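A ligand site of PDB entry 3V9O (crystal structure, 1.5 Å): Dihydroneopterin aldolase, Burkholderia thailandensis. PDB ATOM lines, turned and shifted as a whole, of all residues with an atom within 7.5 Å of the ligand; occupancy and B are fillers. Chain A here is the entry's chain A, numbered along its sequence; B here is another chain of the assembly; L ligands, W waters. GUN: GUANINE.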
ATOM      1  N   ARG A  23       9.707  13.592  34.620  1.00  0.00           N
ATOM      2  CA  ARG A  23      10.445  13.151  33.426  1.00  0.00           C
ATOM      3  C   ARG A  23      10.078  14.035  32.253  1.00  0.00           C
ATOM      4  O   ARG A  23       9.062  14.766  32.284  1.00  0.00           O
ATOM      5  CB  ARG A  23      10.160  11.676  33.094  1.00  0.00           C
ATOM      6  CG  ARG A  23       8.765  11.414  32.588  1.00  0.00           C
ATOM      7  CD  ARG A  23       8.600   9.919  32.156  1.00  0.00           C
ATOM      8  NE  ARG A  23       8.547   8.957  33.293  1.00  0.00           N
ATOM      9  CZ  ARG A  23       9.508   8.082  33.618  1.00  0.00           C
ATOM     10  NH1 ARG A  23      10.654   8.027  33.012  1.00  0.00           N
ATOM     11  NH2 ARG A  23       9.281   7.196  34.581  1.00  0.00           N
ATOM     12  N   LEU A  25       9.239  14.037  28.223  1.00  0.00           N
ATOM     13  CA  LEU A  25       8.920  13.358  26.972  1.00  0.00           C
ATOM     14  C   LEU A  25       9.224  14.361  25.877  1.00  0.00           C
ATOM     15  O   LEU A  25       8.987  15.548  26.064  1.00  0.00           O
ATOM     16  CB  LEU A  25       7.425  13.029  26.947  1.00  0.00           C
ATOM     17  CG  LEU A  25       6.827  12.335  28.200  1.00  0.00           C
ATOM     18  CD1 LEU A  25       5.344  12.121  27.964  1.00  0.00           C
ATOM     19  CD2 LEU A  25       7.491  11.009  28.481  1.00  0.00           C
ATOM     20  N   VAL A  57       6.192  15.644  32.751  1.00  0.00           N
ATOM     21  CA  VAL A  57       5.150  14.909  33.464  1.00  0.00           C
ATOM     22  C   VAL A  57       5.721  14.343  34.785  1.00  0.00           C
ATOM     23  O   VAL A  57       6.877  13.840  34.784  1.00  0.00           O
ATOM     24  CB  VAL A  57       4.543  13.794  32.537  1.00  0.00           C
ATOM     25  CG1 VAL A  57       3.999  14.432  31.268  1.00  0.00           C
ATOM     26  CG2 VAL A  57       5.602  12.768  32.120  1.00  0.00           C
ATOM     27  N   THR A  62       3.959   8.606  36.364  1.00  0.00           N
ATOM     28  CA  THR A  62       4.403   8.009  35.080  1.00  0.00           C
ATOM     29  C   THR A  62       5.532   7.040  35.278  1.00  0.00           C
ATOM     30  O   THR A  62       6.397   6.886  34.406  1.00  0.00           O
ATOM     31  CB  THR A  62       4.862   9.059  34.038  1.00  0.00           C
ATOM     32  OG1 THR A  62       5.994   9.779  34.546  1.00  0.00           O
ATOM     33  CG2 THR A  62       3.714  10.027  33.715  1.00  0.00           C
ATOM     34  N   ASP A  67       5.313  -2.301  33.381  1.00  0.00           N
ATOM     35  CA  ASP A  67       5.623  -2.094  31.957  1.00  0.00           C
ATOM     36  C   ASP A  67       4.352  -2.001  31.084  1.00  0.00           C
ATOM     37  O   ASP A  67       4.348  -2.496  29.959  1.00  0.00           O
ATOM     38  CB  ASP A  67       6.567  -3.186  31.468  1.00  0.00           C
ATOM     39  CG  ASP A  67       7.317  -2.800  30.163  1.00  0.00           C
ATOM     40  OD1 ASP A  67       7.481  -1.623  29.837  1.00  0.00           O
ATOM     41  OD2 ASP A  67       7.791  -3.764  29.532  1.00  0.00           O
ATOM     42  N   LEU A  69       1.308   0.546  29.252  1.00  0.00           N
ATOM     43  CA  LEU A  69       1.110   1.870  28.720  1.00  0.00           C
ATOM     44  C   LEU A  69       0.168   2.700  29.604  1.00  0.00           C
ATOM     45  O   LEU A  69       0.343   3.920  29.713  1.00  0.00           O
ATOM     46  CB  LEU A  69       0.574   1.785  27.268  1.00  0.00           C
ATOM     47  CG  LEU A  69       0.463   3.126  26.547  1.00  0.00           C
ATOM     48  CD1 LEU A  69       1.771   3.951  26.441  1.00  0.00           C
ATOM     49  CD2 LEU A  69      -0.130   2.837  25.126  1.00  0.00           C
ATOM     50  N   VAL A  72       1.654   5.263  32.162  1.00  0.00           N
ATOM     51  CA  VAL A  72       2.368   6.472  31.783  1.00  0.00           C
ATOM     52  C   VAL A  72       1.523   7.418  30.933  1.00  0.00           C
ATOM     53  O   VAL A  72       0.372   7.081  30.537  1.00  0.00           O
ATOM     54  CB  VAL A  72       3.660   6.123  31.007  1.00  0.00           C
ATOM     55  CG1 VAL A  72       4.562   5.190  31.785  1.00  0.00           C
ATOM     56  CG2 VAL A  72       3.392   5.501  29.643  1.00  0.00           C
ATOM     57  N   VAL A  73       2.027   8.625  30.714  1.00  0.00           N
ATOM     58  CA  VAL A  73       1.409   9.566  29.766  1.00  0.00           C
ATOM     59  C   VAL A  73       1.904   9.180  28.371  1.00  0.00           C
ATOM     60  O   VAL A  73       3.086   9.166  28.106  1.00  0.00           O
ATOM     61  CB  VAL A  73       1.795  11.041  30.062  1.00  0.00           C
ATOM     62  CG1 VAL A  73       1.314  11.954  28.921  1.00  0.00           C
ATOM     63  CG2 VAL A  73       1.177  11.484  31.421  1.00  0.00           C
ATOM     64  N   ASP A  74       0.971   8.749  27.517  1.00  0.00           N
ATOM     65  CA  ASP A  74       1.300   8.301  26.160  1.00  0.00           C
ATOM     66  C   ASP A  74       1.922   9.443  25.363  1.00  0.00           C
ATOM     67  O   ASP A  74       1.294  10.494  25.148  1.00  0.00           O
ATOM     68  CB  ASP A  74       0.020   7.830  25.498  1.00  0.00           C
ATOM     69  CG  ASP A  74       0.241   7.099  24.173  1.00  0.00           C
ATOM     70  OD1 ASP A  74       1.223   7.386  23.492  1.00  0.00           O
ATOM     71  OD2 ASP A  74      -0.663   6.286  23.823  1.00  0.00           O
ATOM     72  N   TYR A  75       3.157   9.303  24.929  1.00  0.00           N
ATOM     73  CA  TYR A  75       3.794  10.386  24.237  1.00  0.00           C
ATOM     74  C   TYR A  75       3.269  10.650  22.819  1.00  0.00           C
ATOM     75  O   TYR A  75       3.578  11.721  22.256  1.00  0.00           O
ATOM     76  CB  TYR A  75       5.332  10.199  24.243  1.00  0.00           C
ATOM     77  CG  TYR A  75       5.914   8.939  23.678  1.00  0.00           C
ATOM     78  CD1 TYR A  75       5.487   8.393  22.472  1.00  0.00           C
ATOM     79  CD2 TYR A  75       6.998   8.324  24.315  1.00  0.00           C
ATOM     80  CE1 TYR A  75       6.113   7.245  21.946  1.00  0.00           C
ATOM     81  CE2 TYR A  75       7.620   7.183  23.807  1.00  0.00           C
ATOM     82  CZ  TYR A  75       7.146   6.649  22.620  1.00  0.00           C
ATOM     83  OH  TYR A  75       7.792   5.532  22.140  1.00  0.00           O
ATOM     84  N   ASP A  76       2.380   9.790  22.316  1.00  0.00           N
ATOM     85  CA  ASP A  76       1.673  10.081  21.061  1.00  0.00           C
ATOM     86  C   ASP A  76       0.826  11.371  21.167  1.00  0.00           C
ATOM     87  O   ASP A  76       0.460  11.926  20.130  1.00  0.00           O
ATOM     88  CB  ASP A  76       0.755   8.944  20.623  1.00  0.00           C
ATOM     89  CG  ASP A  76       1.522   7.697  20.110  1.00  0.00           C
ATOM     90  OD1 ASP A  76       2.754   7.716  19.918  1.00  0.00           O
ATOM     91  OD2 ASP A  76       0.811   6.691  19.910  1.00  0.00           O
ATOM     92  N   LEU A  77       0.517  11.811  22.377  1.00  0.00           N
ATOM     93  CA  LEU A  77      -0.218  13.045  22.538  1.00  0.00           C
ATOM     94  C   LEU A  77       0.464  14.244  21.916  1.00  0.00           C
ATOM     95  O   LEU A  77      -0.224  15.152  21.409  1.00  0.00           O
ATOM     96  CB  LEU A  77      -0.471  13.260  24.017  1.00  0.00           C
ATOM     97  CG  LEU A  77      -1.052  14.571  24.462  1.00  0.00           C
ATOM     98  CD1 LEU A  77      -2.560  14.413  24.363  1.00  0.00           C
ATOM     99  CD2 LEU A  77      -0.584  14.917  25.902  1.00  0.00           C
ATOM    100  N   ILE B  36      11.097  -3.675  21.392  1.00  0.00           N
ATOM    101  CA  ILE B  36      10.572  -2.661  22.289  1.00  0.00           C
ATOM    102  C   ILE B  36       9.303  -2.157  21.642  1.00  0.00           C
ATOM    103  O   ILE B  36       9.216  -2.055  20.407  1.00  0.00           O
ATOM    104  CB  ILE B  36      11.537  -1.528  22.517  1.00  0.00           C
ATOM    105  CG1 ILE B  36      10.975  -0.550  23.566  1.00  0.00           C
ATOM    106  CG2 ILE B  36      11.907  -0.804  21.176  1.00  0.00           C
ATOM    107  CD1 ILE B  36      12.059   0.407  24.066  1.00  0.00           C
ATOM    108  N   GLY B  37       8.261  -1.924  22.426  1.00  0.00           N
ATOM    109  CA  GLY B  37       7.034  -1.476  21.820  1.00  0.00           C
ATOM    110  C   GLY B  37       5.918  -1.806  22.747  1.00  0.00           C
ATOM    111  O   GLY B  37       5.866  -2.958  23.238  1.00  0.00           O
ATOM    112  N   ALA B  38       5.053  -0.811  22.972  1.00  0.00           N
ATOM    113  CA  ALA B  38       3.794  -0.968  23.712  1.00  0.00           C
ATOM    114  C   ALA B  38       2.699  -1.541  22.831  1.00  0.00           C
ATOM    115  O   ALA B  38       2.557  -2.756  22.704  1.00  0.00           O
ATOM    116  CB  ALA B  38       3.341   0.361  24.283  1.00  0.00           C
ATOM    117  N   HIS B  92       8.644  -3.203  26.987  1.00  0.00           N
ATOM    118  CA  HIS B  92       7.598  -2.539  26.194  1.00  0.00           C
ATOM    119  C   HIS B  92       7.657  -0.996  26.092  1.00  0.00           C
ATOM    120  O   HIS B  92       7.547  -0.424  24.998  1.00  0.00           O
ATOM    121  CB  HIS B  92       6.247  -2.954  26.727  1.00  0.00           C
ATOM    122  CG  HIS B  92       6.053  -4.427  26.709  1.00  0.00           C
ATOM    123  ND1 HIS B  92       5.395  -5.071  25.687  1.00  0.00           N
ATOM    124  CD2 HIS B  92       6.515  -5.398  27.529  1.00  0.00           C
ATOM    125  CE1 HIS B  92       5.392  -6.375  25.920  1.00  0.00           C
ATOM    126  NE2 HIS B  92       6.076  -6.605  27.036  1.00  0.00           N
ATOM    127  N   LEU B  93       7.869  -0.324  27.227  1.00  0.00           N
ATOM    128  CA  LEU B  93       7.887   1.139  27.260  1.00  0.00           C
ATOM    129  C   LEU B  93       9.284   1.694  27.315  1.00  0.00           C
ATOM    130  O   LEU B  93      10.185   1.139  27.969  1.00  0.00           O
ATOM    131  CB  LEU B  93       7.148   1.613  28.539  1.00  0.00           C
ATOM    132  CG  LEU B  93       5.723   1.196  28.707  1.00  0.00           C
ATOM    133  CD1 LEU B  93       5.208   1.703  30.059  1.00  0.00           C
ATOM    134  CD2 LEU B  93       4.959   1.807  27.572  1.00  0.00           C
ATOM    135  N   GLN B  94       9.496   2.867  26.703  1.00  0.00           N
ATOM    136  CA  GLN B  94      10.758   3.578  26.833  1.00  0.00           C
ATOM    137  C   GLN B  94      11.027   3.910  28.296  1.00  0.00           C
ATOM    138  O   GLN B  94      12.183   3.815  28.719  1.00  0.00           O
ATOM    139  CB  GLN B  94      10.758   4.878  26.018  1.00  0.00           C
ATOM    140  CG  GLN B  94      10.782   4.612  24.495  1.00  0.00           C
ATOM    141  CD  GLN B  94      11.324   5.806  23.739  1.00  0.00           C
ATOM    142  OE1 GLN B  94      12.377   6.348  24.053  1.00  0.00           O
ATOM    143  NE2 GLN B  94      10.615   6.264  22.689  1.00  0.00           N
ATOM    144  N   GLU B  95      10.028   4.279  29.086  1.00  0.00           N
ATOM    145  CA  GLU B  95      10.233   4.585  30.504  1.00  0.00           C
ATOM    146  C   GLU B  95      10.850   3.400  31.223  1.00  0.00           C
ATOM    147  O   GLU B  95      11.720   3.595  32.065  1.00  0.00           O
ATOM    148  CB  GLU B  95       8.920   4.914  31.207  1.00  0.00           C
ATOM    149  CG  GLU B  95       8.353   6.316  30.869  1.00  0.00           C
ATOM    150  CD  GLU B  95       7.570   6.405  29.552  1.00  0.00           C
ATOM    151  OE1 GLU B  95       7.602   5.504  28.679  1.00  0.00           O
ATOM    152  OE2 GLU B  95       6.887   7.423  29.395  1.00  0.00           O
ATOM    153  N   THR B  96      10.417   2.186  30.887  1.00  0.00           N
ATOM    154  CA  THR B  96      10.983   1.007  31.572  1.00  0.00           C
ATOM    155  C   THR B  96      12.488   0.903  31.339  1.00  0.00           C
ATOM    156  O   THR B  96      13.255   0.714  32.288  1.00  0.00           O
ATOM    157  CB  THR B  96      10.271  -0.217  31.110  1.00  0.00           C
ATOM    158  OG1 THR B  96       8.886  -0.097  31.502  1.00  0.00           O
ATOM    159  CG2 THR B  96      10.849  -1.469  31.729  1.00  0.00           C
ATOM    160  N   THR B 118      16.332   7.928  26.310  1.00  0.00           N
ATOM    161  CA  THR B 118      16.144   6.947  25.231  1.00  0.00           C
ATOM    162  C   THR B 118      15.271   7.590  24.172  1.00  0.00           C
ATOM    163  O   THR B 118      14.469   8.467  24.481  1.00  0.00           O
ATOM    164  CB  THR B 118      15.454   5.626  25.738  1.00  0.00           C
ATOM    165  OG1 THR B 118      14.169   5.964  26.256  1.00  0.00           O
ATOM    166  CG2 THR B 118      16.298   4.992  26.908  1.00  0.00           C
ATOM    167  N   LYS B 120      13.343   6.750  20.045  1.00  0.00           N
ATOM    168  CA  LYS B 120      13.109   5.926  18.871  1.00  0.00           C
ATOM    169  C   LYS B 120      13.113   6.788  17.645  1.00  0.00           C
ATOM    170  O   LYS B 120      12.136   7.534  17.359  1.00  0.00           O
ATOM    171  CB  LYS B 120      11.715   5.279  18.986  1.00  0.00           C
ATOM    172  CG  LYS B 120      11.685   4.145  19.924  1.00  0.00           C
ATOM    173  CD  LYS B 120      10.196   3.593  19.971  1.00  0.00           C
ATOM    174  CE  LYS B 120       9.987   2.618  20.985  1.00  0.00           C
ATOM    175  NZ  LYS B 120       8.586   1.997  20.725  1.00  0.00           N
ATOM    176  N   TYR B 124       7.948   7.671  14.091  1.00  0.00           N
ATOM    177  CA  TYR B 124       7.032   8.348  13.186  1.00  0.00           C
ATOM    178  C   TYR B 124       7.774   8.736  11.923  1.00  0.00           C
ATOM    179  O   TYR B 124       8.881   9.310  12.026  1.00  0.00           O
ATOM    180  CB  TYR B 124       6.509   9.660  13.817  1.00  0.00           C
ATOM    181  CG  TYR B 124       5.962   9.557  15.241  1.00  0.00           C
ATOM    182  CD1 TYR B 124       4.829   8.763  15.521  1.00  0.00           C
ATOM    183  CD2 TYR B 124       6.588  10.225  16.279  1.00  0.00           C
ATOM    184  CE1 TYR B 124       4.357   8.656  16.817  1.00  0.00           C
ATOM    185  CE2 TYR B 124       6.088  10.123  17.602  1.00  0.00           C
ATOM    186  CZ  TYR B 124       4.994   9.384  17.834  1.00  0.00           C
ATOM    187  OH  TYR B 124       4.540   9.398  19.150  1.00  0.00           O
ATOM    188  N   VAL B 130      11.172  10.332  18.960  1.00  0.00           N
ATOM    189  CA  VAL B 130      10.392  10.619  20.144  1.00  0.00           C
ATOM    190  C   VAL B 130      11.113   9.872  21.273  1.00  0.00           C
ATOM    191  O   VAL B 130      11.529   8.726  21.091  1.00  0.00           O
ATOM    192  CB  VAL B 130       8.896  10.154  19.967  1.00  0.00           C
ATOM    193  CG1 VAL B 130       8.770   8.646  19.855  1.00  0.00           C
ATOM    194  CG2 VAL B 130       8.004  10.701  21.110  1.00  0.00           C
ATOM    195  N   GLY B 131      11.194  10.527  22.412  1.00  0.00           N
ATOM    196  CA  GLY B 131      11.989   9.980  23.504  1.00  0.00           C
ATOM    197  C   GLY B 131      11.524  10.413  24.852  1.00  0.00           C
ATOM    198  O   GLY B 131      10.566  11.145  25.070  1.00  0.00           O
ATOM    199  N   VAL B 132      12.247   9.819  25.829  1.00  0.00           N
ATOM    200  CA  VAL B 132      12.015   9.985  27.266  1.00  0.00           C
ATOM    201  C   VAL B 132      13.331  10.300  27.967  1.00  0.00           C
ATOM    202  O   VAL B 132      14.351   9.645  27.651  1.00  0.00           O
ATOM    203  CB  VAL B 132      11.400   8.691  27.875  1.00  0.00           C
ATOM    204  CG1 VAL B 132      11.293   8.801  29.447  1.00  0.00           C
ATOM    205  CG2 VAL B 132      10.050   8.400  27.169  1.00  0.00           C
HETATM  206  N9  GUN L   1       3.327   5.454  23.340  1.00  0.00           N
HETATM  207  C8  GUN L   1       3.781   4.342  22.624  1.00  0.00           C
HETATM  208  N7  GUN L   1       4.959   3.785  23.177  1.00  0.00           N
HETATM  209  C5  GUN L   1       5.153   4.568  24.296  1.00  0.00           C
HETATM  210  C6  GUN L   1       6.209   4.538  25.321  1.00  0.00           C
HETATM  211  O6  GUN L   1       7.145   3.714  25.368  1.00  0.00           O
HETATM  212  N1  GUN L   1       6.117   5.503  26.321  1.00  0.00           N
HETATM  213  C2  GUN L   1       5.144   6.503  26.326  1.00  0.00           C
HETATM  214  N2  GUN L   1       5.165   7.471  27.302  1.00  0.00           N
HETATM  215  N3  GUN L   1       4.135   6.551  25.357  1.00  0.00           N
HETATM  216  C4  GUN L   1       4.215   5.574  24.382  1.00  0.00           C
HETATM  217  O   HOH W   1       8.170   1.845  23.447  1.00  0.00           O
HETATM  218  O   HOH W   2       5.581   1.694  21.515  1.00  0.00           O
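N2 of the ligand sits at hydrogen-bond distance from OE2 of Glu 95 of chain B, at 2.7 Å. A nitrogen (N3) of the ligand is in hydrogen-bond range of the backbone NH (N) of Tyr 75, at 3.0 Å. The backbone NH (N) of Gln 94 of chain B lies within hydrogen-bond range of an oxygen (O6) of the ligand (2.8 Å). OD1 of Asp 74 is in hydrogen-bond range of N9 of the ligand (2.9 Å). O of Val 73 is in hydrogen-bond range of N2 of the ligand (2.8 Å). The side-chain hydroxyl (OH) of Tyr 75 lies within hydrogen-bond range of a nitrogen (N7) of the ligand (3.5 Å).
Water W2 lies within hydrogen-bond range of a nitrogen (N7) of the ligand (2.7 Å), the backbone NH of Ala 38 of chain B (2.9 Å) and the side-chain amino group of Lys 120 of chain B (3.1 Å). Water W1 lies within hydrogen-bond range of NZ of Lys 120 of chain B (2.8 Å), O of His 92 of chain B (2.8 Å) and O6 of the ligand (2.9 Å).
The side-chain carboxylate of Asp 67 lies within hydrogen-bond range of the backbone NH of Leu 93 of chain B (2.9 Å). OD1 of Asp 74 sits at hydrogen-bond distance from N of Asp 76, 2.9 Å away. The backbone NH (N) of Ala 38 of chain B lies within hydrogen-bond range of the backbone carbonyl oxygen (O) of His 92 of chain B, 3.2 Å away. The side-chain amide oxygen of Gln 94 of chain B is in hydrogen-bond range of the side-chain hydroxyl of Thr 118 of chain B, at 2.9 Å. The side-chain hydroxyl of Tyr 75 sits at hydrogen-bond distance from the side-chain amide nitrogen of Gln 94 of chain B, 3.0 Å away. The backbone carbonyl oxygen of Val 130 of chain B is in hydrogen-bond range of the side-chain amide nitrogen of Gln 94 of chain B (3.1 Å).
Merely in contact with the ligand: Leu 69 (3.6 Å), Val 72 (3.5 Å), Ala 38 of chain B (3.9 Å) and Leu 93 of chain B (3.3 Å). Hydrophobic or aromatic side chains within 4 Å of the ligand: Leu 69, Val 72, Tyr 75, Ala 38 of chain B and Leu 93 of chain B. Within 4 Å of the ligand: Leu 69, Val 72, Val 73, Asp 74, Tyr 75, Ala 38 of chain B, Leu 93 of chain B, Gln 94 of chain B and Glu 95 of chain B.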
